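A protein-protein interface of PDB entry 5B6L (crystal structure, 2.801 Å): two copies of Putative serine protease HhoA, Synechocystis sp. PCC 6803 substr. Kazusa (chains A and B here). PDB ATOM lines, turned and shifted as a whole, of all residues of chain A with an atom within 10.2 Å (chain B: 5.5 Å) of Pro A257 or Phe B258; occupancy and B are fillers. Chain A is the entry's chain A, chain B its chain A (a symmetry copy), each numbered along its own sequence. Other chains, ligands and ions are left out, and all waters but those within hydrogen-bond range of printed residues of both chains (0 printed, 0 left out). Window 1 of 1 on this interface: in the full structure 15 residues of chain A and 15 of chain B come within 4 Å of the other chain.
NH1 of Arg A284 lies close to N of Pro B257 (3.4 Å).
NH2 of Arg A283 is in hydrogen-bond range of OG of Ser B256, at 3.3 Å.
NH1 of Arg B284 lies close to N of Pro A257.
NH1 of Arg B283 sits at hydrogen-bond distance from O of Asn A253 (3.0 Å).
The side-chain hydroxyl of Ser A256 is in hydrogen-bond range of the guanidinium group of Arg B283, 3.3 Å away.
O of Pro A254 is in hydrogen-bond range of N of Arg B284, 2.7 Å away.
The side-chain amide nitrogen (ND2) of Asn B251 lies within hydrogen-bond range of the backbone carbonyl oxygen (O) of Ile B260 (2.4 Å).
ND2 of Asn A250 is in hydrogen-bond range of OG of Ser A256 (3.3 Å).
The side-chain amide nitrogen (ND2) of Asn A251 is in hydrogen-bond range of the backbone carbonyl oxygen (O) of Ile A260, 2.4 Å away.
The backbone carbonyl oxygen (O) of Asn A253 lies within hydrogen-bond range of the side-chain hydroxyl (OG) of Ser A256, at 3.3 Å.
ND2 of Asn B250 is in hydrogen-bond range of OG of Ser B256 (3.3 Å).
N of Asn A255 lies close to OD1 of Asn A253, at 3.2 Å.
O of Asn A251 touches NH1 of Arg B283, 3.96 Å away.
Arg B283 touches Pro A254 (CA to O, 3.6 Å).
NH1 of Arg B284 touches O of Asn A255, 3.6 Å away.
Ser A256 touches Arg B284.
Pro A257 touches Phe B258 (O to CD2, 3.5 Å).
CD2 of Phe A258 touches O of Pro B257 (3.5 Å).
Arg B283 touches Ile A259.
Asn B251 touches Arg A283.
Ile B259 touches Arg A283 (CG2 to NH2, 3.4 Å).
Arg A284 touches Ser B256.
Pro A257 touches just these residues of chain B: Phe B258 and Arg B284.
Of chain A, only Pro A257 (3.5 Å) comes within 4 Å of Phe B258.
Ser B256 touches just these residues of chain A: Arg A283 (3.3 Å) and Arg A284 (3.9 Å).
Pro B257 touches just these residues of chain A: Phe A258 (3.5 Å) and Arg A284 (3.3 Å).
Ile B259 touches just one residue of chain A: Arg A283 (3.4 Å).
Ile B260 touches none of the printed residues of chain A.
Of the printed residues of chain B, Ser A256 touches Arg B283 and Arg B284.
Printed residues of chain B within 4 Å of Phe A258: Pro B257 (3.5 Å).
Of the printed residues of chain B, Pro A254 touches Arg B283 and Arg B284.
Of the printed residues of chain B, Asn A251 touches Arg B283 (3.96 Å).
The nearest residue of chain B that does not touch Pro A257 is Pro B257 (4.2 Å).
Of the 24 printed residues of chain A, 10 touch a printed residue of chain B.
Of the 13 printed residues of chain B, 7 touch a printed residue of chain A.
Hydrophobic or aromatic side chains of chain B within 4 Å of the printed part of chain A: Pro B257, Phe B258 and Ile B259.
Among the printed residues, 16 pairs touch across the chains.
Among the printed residues, no Asp or Glu carboxylate lies within 4 Å of a Lys or Arg side-chain nitrogen of the other chain.
Ser A256 touches Arg B284, and with the chains exchanged Arg A284 touches Ser B256.
Pro A257 touches Phe B258, and with the chains exchanged Phe A258 touches Pro B257.
Pro A257 touches Arg B284, and with the chains exchanged Arg A284 touches Pro B257.
Ile A259 touches Arg B283, and with the chains exchanged Arg A283 touches Ile B259.
13 positions are printed for both chains.
Of the 16 pairs that touch across the chains among the printed residues, 12 have their exchanged pair printed and touching as well.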
ATOM      1  N   GLN A 246       1.749 -18.143  10.631  1.00  0.00           N
ATOM      2  CA  GLN A 246       2.720 -17.239  10.018  1.00  0.00           C
ATOM      3  C   GLN A 246       3.245 -16.264  11.078  1.00  0.00           C
ATOM      4  O   GLN A 246       4.427 -15.922  11.076  1.00  0.00           O
ATOM      5  CB  GLN A 246       2.090 -16.445   8.871  1.00  0.00           C
ATOM      6  CG  GLN A 246       2.084 -17.108   7.510  1.00  0.00           C
ATOM      7  CD  GLN A 246       1.393 -16.238   6.479  1.00  0.00           C
ATOM      8  OE1 GLN A 246       0.341 -15.662   6.758  1.00  0.00           O
ATOM      9  NE2 GLN A 246       1.997 -16.105   5.296  1.00  0.00           N
ATOM     10  N   ALA A 247       2.360 -15.825  11.974  1.00  0.00           N
ATOM     11  CA  ALA A 247       2.699 -14.886  13.045  1.00  0.00           C
ATOM     12  C   ALA A 247       3.713 -15.431  14.060  1.00  0.00           C
ATOM     13  O   ALA A 247       4.831 -14.908  14.209  1.00  0.00           O
ATOM     14  CB  ALA A 247       1.426 -14.465  13.760  1.00  0.00           C
ATOM     15  N   GLN A 249       5.192 -17.965  13.840  1.00  0.00           N
ATOM     16  CA  GLN A 249       6.294 -18.455  13.053  1.00  0.00           C
ATOM     17  C   GLN A 249       7.242 -17.310  12.734  1.00  0.00           C
ATOM     18  O   GLN A 249       8.461 -17.492  12.683  1.00  0.00           O
ATOM     19  CB  GLN A 249       5.766 -19.072  11.775  1.00  0.00           C
ATOM     20  CG  GLN A 249       6.822 -19.362  10.751  1.00  0.00           C
ATOM     21  CD  GLN A 249       6.285 -20.213   9.645  1.00  0.00           C
ATOM     22  OE1 GLN A 249       6.169 -21.427   9.793  1.00  0.00           O
ATOM     23  NE2 GLN A 249       5.927 -19.585   8.529  1.00  0.00           N
ATOM     24  N   ASN A 250       6.674 -16.128  12.509  1.00  0.00           N
ATOM     25  CA  ASN A 250       7.473 -14.918  12.357  1.00  0.00           C
ATOM     26  C   ASN A 250       8.200 -14.657  13.664  1.00  0.00           C
ATOM     27  O   ASN A 250       9.422 -14.500  13.691  1.00  0.00           O
ATOM     28  CB  ASN A 250       6.587 -13.720  11.986  1.00  0.00           C
ATOM     29  CG  ASN A 250       7.332 -12.389  12.041  1.00  0.00           C
ATOM     30  OD1 ASN A 250       7.886 -11.933  11.039  1.00  0.00           O
ATOM     31  ND2 ASN A 250       7.327 -11.752  13.210  1.00  0.00           N
ATOM     32  N   ASN A 251       7.432 -14.654  14.751  1.00  0.00           N
ATOM     33  CA  ASN A 251       7.941 -14.418  16.099  1.00  0.00           C
ATOM     34  C   ASN A 251       9.033 -15.379  16.585  1.00  0.00           C
ATOM     35  O   ASN A 251       9.521 -15.237  17.704  1.00  0.00           O
ATOM     36  CB  ASN A 251       6.787 -14.432  17.099  1.00  0.00           C
ATOM     37  CG  ASN A 251       5.744 -13.389  16.792  1.00  0.00           C
ATOM     38  OD1 ASN A 251       5.737 -12.806  15.710  1.00  0.00           O
ATOM     39  ND2 ASN A 251       4.853 -13.142  17.744  1.00  0.00           N
ATOM     40  N   ARG A 252       9.410 -16.358  15.767  1.00  0.00           N
ATOM     41  CA  ARG A 252      10.497 -17.253  16.146  1.00  0.00           C
ATOM     42  C   ARG A 252      11.703 -17.093  15.226  1.00  0.00           C
ATOM     43  O   ARG A 252      12.732 -17.744  15.410  1.00  0.00           O
ATOM     44  CB  ARG A 252      10.038 -18.717  16.226  1.00  0.00           C
ATOM     45  CG  ARG A 252       9.800 -19.411  14.893  1.00  0.00           C
ATOM     46  CD  ARG A 252       9.624 -20.919  15.091  1.00  0.00           C
ATOM     47  NE  ARG A 252       8.657 -21.229  16.141  1.00  0.00           N
ATOM     48  CZ  ARG A 252       7.371 -21.479  15.922  1.00  0.00           C
ATOM     49  NH1 ARG A 252       6.891 -21.460  14.682  1.00  0.00           N
ATOM     50  NH2 ARG A 252       6.565 -21.750  16.942  1.00  0.00           N
ATOM     51  N   ASN A 253      11.564 -16.220  14.233  1.00  0.00           N
ATOM     52  CA  ASN A 253      12.702 -15.778  13.437  1.00  0.00           C
ATOM     53  C   ASN A 253      13.359 -14.603  14.148  1.00  0.00           C
ATOM     54  O   ASN A 253      12.746 -13.548  14.304  1.00  0.00           O
ATOM     55  CB  ASN A 253      12.241 -15.360  12.046  1.00  0.00           C
ATOM     56  CG  ASN A 253      13.386 -14.935  11.150  1.00  0.00           C
ATOM     57  OD1 ASN A 253      14.561 -15.048  11.507  1.00  0.00           O
ATOM     58  ND2 ASN A 253      13.045 -14.454   9.962  1.00  0.00           N
ATOM     59  N   PRO A 254      14.605 -14.785  14.603  1.00  0.00           N
ATOM     60  CA  PRO A 254      15.287 -13.728  15.352  1.00  0.00           C
ATOM     61  C   PRO A 254      15.463 -12.431  14.555  1.00  0.00           C
ATOM     62  O   PRO A 254      15.623 -11.372  15.153  1.00  0.00           O
ATOM     63  CB  PRO A 254      16.649 -14.356  15.681  1.00  0.00           C
ATOM     64  CG  PRO A 254      16.814 -15.466  14.716  1.00  0.00           C
ATOM     65  CD  PRO A 254      15.437 -15.989  14.475  1.00  0.00           C
ATOM     66  N   ASN A 255      15.409 -12.507  13.230  1.00  0.00           N
ATOM     67  CA  ASN A 255      15.623 -11.326  12.400  1.00  0.00           C
ATOM     68  C   ASN A 255      14.376 -10.818  11.673  1.00  0.00           C
ATOM     69  O   ASN A 255      14.468 -10.193  10.620  1.00  0.00           O
ATOM     70  CB  ASN A 255      16.786 -11.556  11.431  1.00  0.00           C
ATOM     71  CG  ASN A 255      18.126 -11.641  12.150  1.00  0.00           C
ATOM     72  OD1 ASN A 255      18.515 -10.722  12.864  1.00  0.00           O
ATOM     73  ND2 ASN A 255      18.825 -12.753  11.978  1.00  0.00           N
ATOM     74  N   SER A 256      13.208 -11.081  12.242  1.00  0.00           N
ATOM     75  CA  SER A 256      11.992 -10.458  11.747  1.00  0.00           C
ATOM     76  C   SER A 256      11.903  -9.038  12.318  1.00  0.00           C
ATOM     77  O   SER A 256      12.311  -8.802  13.459  1.00  0.00           O
ATOM     78  CB  SER A 256      10.768 -11.282  12.147  1.00  0.00           C
ATOM     79  OG  SER A 256      10.523 -11.194  13.538  1.00  0.00           O
ATOM     80  N   PRO A 257      11.379  -8.086  11.524  1.00  0.00           N
ATOM     81  CA  PRO A 257      11.276  -6.670  11.907  1.00  0.00           C
ATOM     82  C   PRO A 257      10.589  -6.466  13.250  1.00  0.00           C
ATOM     83  O   PRO A 257      11.163  -5.880  14.167  1.00  0.00           O
ATOM     84  CB  PRO A 257      10.409  -6.077  10.793  1.00  0.00           C
ATOM     85  CG  PRO A 257      10.699  -6.923   9.617  1.00  0.00           C
ATOM     86  CD  PRO A 257      10.879  -8.316  10.157  1.00  0.00           C
ATOM     87  N   PHE A 258       9.364  -6.957  13.357  1.00  0.00           N
ATOM     88  CA  PHE A 258       8.584  -6.798  14.570  1.00  0.00           C
ATOM     89  C   PHE A 258       7.864  -8.097  14.881  1.00  0.00           C
ATOM     90  O   PHE A 258       7.480  -8.828  13.970  1.00  0.00           O
ATOM     91  CB  PHE A 258       7.565  -5.679  14.377  1.00  0.00           C
ATOM     92  CG  PHE A 258       6.797  -5.778  13.089  1.00  0.00           C
ATOM     93  CD1 PHE A 258       5.635  -6.524  13.014  1.00  0.00           C
ATOM     94  CD2 PHE A 258       7.239  -5.123  11.950  1.00  0.00           C
ATOM     95  CE1 PHE A 258       4.932  -6.616  11.830  1.00  0.00           C
ATOM     96  CE2 PHE A 258       6.538  -5.213  10.763  1.00  0.00           C
ATOM     97  CZ  PHE A 258       5.385  -5.960  10.702  1.00  0.00           C
ATOM     98  N   ILE A 259       7.681  -8.396  16.162  1.00  0.00           N
ATOM     99  CA  ILE A 259       6.867  -9.548  16.528  1.00  0.00           C
ATOM    100  C   ILE A 259       5.387  -9.239  16.291  1.00  0.00           C
ATOM    101  O   ILE A 259       4.867  -8.215  16.746  1.00  0.00           O
ATOM    102  CB  ILE A 259       7.142 -10.061  17.978  1.00  0.00           C
ATOM    103  CG1 ILE A 259       6.399  -9.241  19.039  1.00  0.00           C
ATOM    104  CG2 ILE A 259       8.635 -10.106  18.258  1.00  0.00           C
ATOM    105  CD1 ILE A 259       6.843  -7.795  19.152  1.00  0.00           C
ATOM    106  N   ILE A 260       4.723 -10.097  15.524  1.00  0.00           N
ATOM    107  CA  ILE A 260       3.285  -9.973  15.352  1.00  0.00           C
ATOM    108  C   ILE A 260       2.644 -10.547  16.603  1.00  0.00           C
ATOM    109  O   ILE A 260       3.088 -11.577  17.107  1.00  0.00           O
ATOM    110  CB  ILE A 260       2.773 -10.719  14.105  1.00  0.00           C
ATOM    111  CG1 ILE A 260       3.255 -10.035  12.829  1.00  0.00           C
ATOM    112  CG2 ILE A 260       1.263 -10.753  14.087  1.00  0.00           C
ATOM    113  CD1 ILE A 260       4.483 -10.651  12.230  1.00  0.00           C
ATOM    114  N   PRO A 261       1.628  -9.859  17.136  1.00  0.00           N
ATOM    115  CA  PRO A 261       0.904 -10.314  18.327  1.00  0.00           C
ATOM    116  C   PRO A 261       0.037 -11.541  18.058  1.00  0.00           C
ATOM    117  O   PRO A 261      -1.181 -11.470  18.237  1.00  0.00           O
ATOM    118  CB  PRO A 261       0.018  -9.115  18.678  1.00  0.00           C
ATOM    119  CG  PRO A 261       0.676  -7.948  18.031  1.00  0.00           C
ATOM    120  CD  PRO A 261       1.267  -8.482  16.770  1.00  0.00           C
ATOM    121  N   LEU A 267      -2.000  -7.428   8.623  1.00  0.00           N
ATOM    122  CA  LEU A 267      -0.822  -6.792   9.175  1.00  0.00           C
ATOM    123  C   LEU A 267      -0.522  -5.579   8.312  1.00  0.00           C
ATOM    124  O   LEU A 267      -0.178  -5.721   7.137  1.00  0.00           O
ATOM    125  CB  LEU A 267       0.327  -7.786   9.219  1.00  0.00           C
ATOM    126  CG  LEU A 267       1.612  -7.207   9.790  1.00  0.00           C
ATOM    127  CD1 LEU A 267       1.407  -6.826  11.241  1.00  0.00           C
ATOM    128  CD2 LEU A 267       2.726  -8.210   9.644  1.00  0.00           C
ATOM    129  N   VAL A 268      -0.652  -4.390   8.900  1.00  0.00           N
ATOM    130  CA  VAL A 268      -0.282  -3.144   8.237  1.00  0.00           C
ATOM    131  C   VAL A 268       1.191  -3.267   7.854  1.00  0.00           C
ATOM    132  O   VAL A 268       2.059  -3.358   8.716  1.00  0.00           O
ATOM    133  CB  VAL A 268      -0.554  -1.921   9.137  1.00  0.00           C
ATOM    134  CG1 VAL A 268      -0.390  -0.636   8.347  1.00  0.00           C
ATOM    135  CG2 VAL A 268      -1.954  -1.992   9.731  1.00  0.00           C
ATOM    136  N   MET A 269       1.460  -3.290   6.552  1.00  0.00           N
ATOM    137  CA  MET A 269       2.812  -3.505   6.049  1.00  0.00           C
ATOM    138  C   MET A 269       3.446  -2.157   5.791  1.00  0.00           C
ATOM    139  O   MET A 269       4.669  -2.012   5.829  1.00  0.00           O
ATOM    140  CB  MET A 269       2.818  -4.298   4.743  1.00  0.00           C
ATOM    141  CG  MET A 269       2.264  -5.695   4.856  1.00  0.00           C
ATOM    142  SD  MET A 269       3.393  -6.768   5.753  1.00  0.00           S
ATOM    143  CE  MET A 269       4.934  -6.410   4.908  1.00  0.00           C
ATOM    144  N   ARG A 283       0.540   2.968  12.395  1.00  0.00           N
ATOM    145  CA  ARG A 283       1.939   2.672  12.144  1.00  0.00           C
ATOM    146  C   ARG A 283       2.111   1.358  11.407  1.00  0.00           C
ATOM    147  O   ARG A 283       1.231   0.504  11.421  1.00  0.00           O
ATOM    148  CB  ARG A 283       2.698   2.574  13.461  1.00  0.00           C
ATOM    149  CG  ARG A 283       2.908   3.880  14.176  1.00  0.00           C
ATOM    150  CD  ARG A 283       3.795   3.655  15.387  1.00  0.00           C
ATOM    151  NE  ARG A 283       4.858   2.691  15.105  1.00  0.00           N
ATOM    152  CZ  ARG A 283       6.024   3.007  14.549  1.00  0.00           C
ATOM    153  NH1 ARG A 283       6.278   4.268  14.207  1.00  0.00           N
ATOM    154  NH2 ARG A 283       6.934   2.064  14.326  1.00  0.00           N
ATOM    155  N   ARG A 284       3.265   1.200  10.774  1.00  0.00           N
ATOM    156  CA  ARG A 284       3.667  -0.077  10.222  1.00  0.00           C
ATOM    157  C   ARG A 284       3.773  -1.087  11.357  1.00  0.00           C
ATOM    158  O   ARG A 284       4.197  -0.751  12.463  1.00  0.00           O
ATOM    159  CB  ARG A 284       5.017   0.062   9.517  1.00  0.00           C
ATOM    160  CG  ARG A 284       5.614  -1.244   9.040  1.00  0.00           C
ATOM    161  CD  ARG A 284       7.026  -1.060   8.523  1.00  0.00           C
ATOM    162  NE  ARG A 284       7.611  -2.334   8.115  1.00  0.00           N
ATOM    163  CZ  ARG A 284       8.910  -2.533   7.917  1.00  0.00           C
ATOM    164  NH1 ARG A 284       9.771  -1.539   8.093  1.00  0.00           N
ATOM    165  NH2 ARG A 284       9.351  -3.733   7.548  1.00  0.00           N
ATOM    166  N   GLY A 285       3.380  -2.324  11.089  1.00  0.00           N
ATOM    167  CA  GLY A 285       3.476  -3.374  12.084  1.00  0.00           C
ATOM    168  C   GLY A 285       2.213  -3.506  12.907  1.00  0.00           C
ATOM    169  O   GLY A 285       2.049  -4.469  13.646  1.00  0.00           O
ATOM    170  N   ASP A 286       1.320  -2.533  12.781  1.00  0.00           N
ATOM    171  CA  ASP A 286       0.058  -2.577  13.498  1.00  0.00           C
ATOM    172  C   ASP A 286      -0.821  -3.692  12.960  1.00  0.00           C
ATOM    173  O   ASP A 286      -0.638  -4.157  11.835  1.00  0.00           O
ATOM    174  CB  ASP A 286      -0.667  -1.233  13.408  1.00  0.00           C
ATOM    175  CG  ASP A 286      -0.026  -0.166  14.277  1.00  0.00           C
ATOM    176  OD1 ASP A 286       1.093  -0.398  14.787  1.00  0.00           O
ATOM    177  OD2 ASP A 286      -0.634   0.910  14.447  1.00  0.00           O
ATOM    178  N   ARG A 321      -0.983  -2.696  18.998  1.00  0.00           N
ATOM    179  CA  ARG A 321       0.392  -2.340  18.681  1.00  0.00           C
ATOM    180  C   ARG A 321       1.353  -3.145  19.553  1.00  0.00           C
ATOM    181  O   ARG A 321       1.765  -2.697  20.628  1.00  0.00           O
ATOM    182  CB  ARG A 321       0.590  -0.843  18.903  1.00  0.00           C
ATOM    183  CG  ARG A 321       1.906  -0.302  18.411  1.00  0.00           C
ATOM    184  CD  ARG A 321       1.816   1.200  18.238  1.00  0.00           C
ATOM    185  NE  ARG A 321       0.919   1.557  17.150  1.00  0.00           N
ATOM    186  CZ  ARG A 321       0.628   2.805  16.806  1.00  0.00           C
ATOM    187  NH1 ARG A 321       1.160   3.816  17.476  1.00  0.00           N
ATOM    188  NH2 ARG A 321      -0.200   3.044  15.798  1.00  0.00           N
ATOM    189  N   GLY A 322       1.698  -4.341  19.088  1.00  0.00           N
ATOM    190  CA  GLY A 322       2.490  -5.266  19.876  1.00  0.00           C
ATOM    191  C   GLY A 322       1.702  -5.801  21.060  1.00  0.00           C
ATOM    192  O   GLY A 322       1.160  -6.908  21.013  1.00  0.00           O
ATOM    193  N   ASN B 250      13.225   8.069  14.806  1.00  0.00           N
ATOM    194  CA  ASN B 250      12.758   6.844  14.167  1.00  0.00           C
ATOM    195  C   ASN B 250      11.311   6.616  14.568  1.00  0.00           C
ATOM    196  O   ASN B 250      10.437   6.444  13.718  1.00  0.00           O
ATOM    197  CB  ASN B 250      13.626   5.647  14.581  1.00  0.00           C
ATOM    198  CG  ASN B 250      13.049   4.309  14.130  1.00  0.00           C
ATOM    199  OD1 ASN B 250      13.371   3.812  13.049  1.00  0.00           O
ATOM    200  ND2 ASN B 250      12.206   3.710  14.971  1.00  0.00           N
ATOM    201  N   ASN B 251      11.070   6.659  15.877  1.00  0.00           N
ATOM    202  CA  ASN B 251       9.747   6.460  16.460  1.00  0.00           C
ATOM    203  C   ASN B 251       8.650   7.421  15.988  1.00  0.00           C
ATOM    204  O   ASN B 251       7.506   7.309  16.424  1.00  0.00           O
ATOM    205  CB  ASN B 251       9.838   6.522  17.983  1.00  0.00           C
ATOM    206  CG  ASN B 251      10.772   5.484  18.550  1.00  0.00           C
ATOM    207  OD1 ASN B 251      11.543   4.867  17.819  1.00  0.00           O
ATOM    208  ND2 ASN B 251      10.710   5.281  19.859  1.00  0.00           N
ATOM    209  N   SER B 256       8.782   2.928  10.109  1.00  0.00           N
ATOM    210  CA  SER B 256       9.977   2.306  10.654  1.00  0.00           C
ATOM    211  C   SER B 256       9.611   0.906  11.162  1.00  0.00           C
ATOM    212  O   SER B 256       8.506   0.702  11.674  1.00  0.00           O
ATOM    213  CB  SER B 256      10.557   3.159  11.782  1.00  0.00           C
ATOM    214  OG  SER B 256       9.731   3.119  12.931  1.00  0.00           O
ATOM    215  N   PRO B 257      10.532  -0.064  11.014  1.00  0.00           N
ATOM    216  CA  PRO B 257      10.311  -1.465  11.400  1.00  0.00           C
ATOM    217  C   PRO B 257       9.827  -1.616  12.836  1.00  0.00           C
ATOM    218  O   PRO B 257       8.762  -2.179  13.085  1.00  0.00           O
ATOM    219  CB  PRO B 257      11.705  -2.082  11.263  1.00  0.00           C
ATOM    220  CG  PRO B 257      12.356  -1.279  10.207  1.00  0.00           C
ATOM    221  CD  PRO B 257      11.863   0.129  10.410  1.00  0.00           C
ATOM    222  N   PHE B 258      10.613  -1.105  13.772  1.00  0.00           N
ATOM    223  CA  PHE B 258      10.288  -1.214  15.181  1.00  0.00           C
ATOM    224  C   PHE B 258      10.586   0.105  15.871  1.00  0.00           C
ATOM    225  O   PHE B 258      11.516   0.810  15.486  1.00  0.00           O
ATOM    226  CB  PHE B 258      11.123  -2.324  15.811  1.00  0.00           C
ATOM    227  CG  PHE B 258      12.581  -2.257  15.459  1.00  0.00           C
ATOM    228  CD1 PHE B 258      13.457  -1.498  16.214  1.00  0.00           C
ATOM    229  CD2 PHE B 258      13.079  -2.954  14.370  1.00  0.00           C
ATOM    230  CE1 PHE B 258      14.797  -1.435  15.887  1.00  0.00           C
ATOM    231  CE2 PHE B 258      14.419  -2.894  14.039  1.00  0.00           C
ATOM    232  CZ  PHE B 258      15.278  -2.134  14.798  1.00  0.00           C
ATOM    233  N   ILE B 259       9.802   0.447  16.886  1.00  0.00           N
ATOM    234  CA  ILE B 259      10.124   1.622  17.686  1.00  0.00           C
ATOM    235  C   ILE B 259      11.323   1.325  18.590  1.00  0.00           C
ATOM    236  O   ILE B 259      11.347   0.324  19.313  1.00  0.00           O
ATOM    237  CB  ILE B 259       8.901   2.178  18.485  1.00  0.00           C
ATOM    238  CG1 ILE B 259       8.650   1.403  19.784  1.00  0.00           C
ATOM    239  CG2 ILE B 259       7.659   2.211  17.611  1.00  0.00           C
ATOM    240  CD1 ILE B 259       8.240  -0.045  19.592  1.00  0.00           C
ATOM    241  N   ILE B 260      12.348   2.167  18.502  1.00  0.00           N
ATOM    242  CA  ILE B 260      13.474   2.057  19.415  1.00  0.00           C
ATOM    243  C   ILE B 260      13.035   2.680  20.728  1.00  0.00           C
ATOM    244  O   ILE B 260      12.378   3.720  20.729  1.00  0.00           O
ATOM    245  CB  ILE B 260      14.733   2.769  18.886  1.00  0.00           C
ATOM    246  CG1 ILE B 260      15.300   2.038  17.674  1.00  0.00           C
ATOM    247  CG2 ILE B 260      15.802   2.823  19.953  1.00  0.00           C
ATOM    248  CD1 ILE B 260      14.879   2.617  16.356  1.00  0.00           C
ATOM    249  N   LEU B 267      21.945  -0.633  18.582  1.00  0.00           N
ATOM    250  CA  LEU B 267      20.718  -1.266  18.145  1.00  0.00           C
ATOM    251  C   LEU B 267      21.109  -2.511  17.368  1.00  0.00           C
ATOM    252  O   LEU B 267      21.712  -2.412  16.297  1.00  0.00           O
ATOM    253  CB  LEU B 267      19.897  -0.287  17.322  1.00  0.00           C
ATOM    254  CG  LEU B 267      18.584  -0.865  16.819  1.00  0.00           C
ATOM    255  CD1 LEU B 267      17.683  -1.196  17.991  1.00  0.00           C
ATOM    256  CD2 LEU B 267      17.923   0.117  15.889  1.00  0.00           C
ATOM    257  N   VAL B 268      20.763  -3.678  17.910  1.00  0.00           N
ATOM    258  CA  VAL B 268      20.962  -4.950  17.222  1.00  0.00           C
ATOM    259  C   VAL B 268      20.209  -4.860  15.897  1.00  0.00           C
ATOM    260  O   VAL B 268      18.986  -4.753  15.875  1.00  0.00           O
ATOM    261  CB  VAL B 268      20.491  -6.139  18.086  1.00  0.00           C
ATOM    262  CG1 VAL B 268      20.924  -7.451  17.458  1.00  0.00           C
ATOM    263  CG2 VAL B 268      21.045  -6.030  19.499  1.00  0.00           C
ATOM    264  N   MET B 269      20.952  -4.882  14.796  1.00  0.00           N
ATOM    265  CA  MET B 269      20.371  -4.703  13.471  1.00  0.00           C
ATOM    266  C   MET B 269      20.094  -6.067  12.881  1.00  0.00           C
ATOM    267  O   MET B 269      19.211  -6.228  12.037  1.00  0.00           O
ATOM    268  CB  MET B 269      21.312  -3.953  12.529  1.00  0.00           C
ATOM    269  CG  MET B 269      21.637  -2.545  12.959  1.00  0.00           C
ATOM    270  SD  MET B 269      20.221  -1.459  12.742  1.00  0.00           S
ATOM    271  CE  MET B 269      19.745  -1.866  11.061  1.00  0.00           C
ATOM    272  N   ARG B 283      17.330 -10.934  19.735  1.00  0.00           N
ATOM    273  CA  ARG B 283      16.536 -10.666  18.549  1.00  0.00           C
ATOM    274  C   ARG B 283      16.961  -9.379  17.869  1.00  0.00           C
ATOM    275  O   ARG B 283      17.576  -8.513  18.481  1.00  0.00           O
ATOM    276  CB  ARG B 283      15.064 -10.536  18.923  1.00  0.00           C
ATOM    277  CG  ARG B 283      14.388 -11.820  19.314  1.00  0.00           C
ATOM    278  CD  ARG B 283      12.906 -11.568  19.517  1.00  0.00           C
ATOM    279  NE  ARG B 283      12.378 -10.629  18.528  1.00  0.00           N
ATOM    280  CZ  ARG B 283      11.957 -10.979  17.316  1.00  0.00           C
ATOM    281  NH1 ARG B 283      12.007 -12.253  16.937  1.00  0.00           N
ATOM    282  NH2 ARG B 283      11.494 -10.056  16.479  1.00  0.00           N
ATOM    283  N   ARG B 284      16.610  -9.257  16.596  1.00  0.00           N
ATOM    284  CA  ARG B 284      16.741  -8.004  15.882  1.00  0.00           C
ATOM    285  C   ARG B 284      15.869  -6.960  16.566  1.00  0.00           C
ATOM    286  O   ARG B 284      14.777  -7.266  17.045  1.00  0.00           O
ATOM    287  CB  ARG B 284      16.300  -8.185  14.429  1.00  0.00           C
ATOM    288  CG  ARG B 284      16.243  -6.903  13.626  1.00  0.00           C
ATOM    289  CD  ARG B 284      15.623  -7.123  12.261  1.00  0.00           C
ATOM    290  NE  ARG B 284      15.524  -5.871  11.517  1.00  0.00           N
ATOM    291  CZ  ARG B 284      14.761  -5.696  10.442  1.00  0.00           C
ATOM    292  NH1 ARG B 284      14.020  -6.696   9.982  1.00  0.00           N
ATOM    293  NH2 ARG B 284      14.734  -4.516   9.831  1.00  0.00           N
ATOM    294  N   GLY B 285      16.352  -5.726  16.620  1.00  0.00           N
ATOM    295  CA  GLY B 285      15.587  -4.647  17.212  1.00  0.00           C
ATOM    296  C   GLY B 285      15.883  -4.470  18.685  1.00  0.00           C
ATOM    297  O   GLY B 285      15.482  -3.482  19.287  1.00  0.00           O
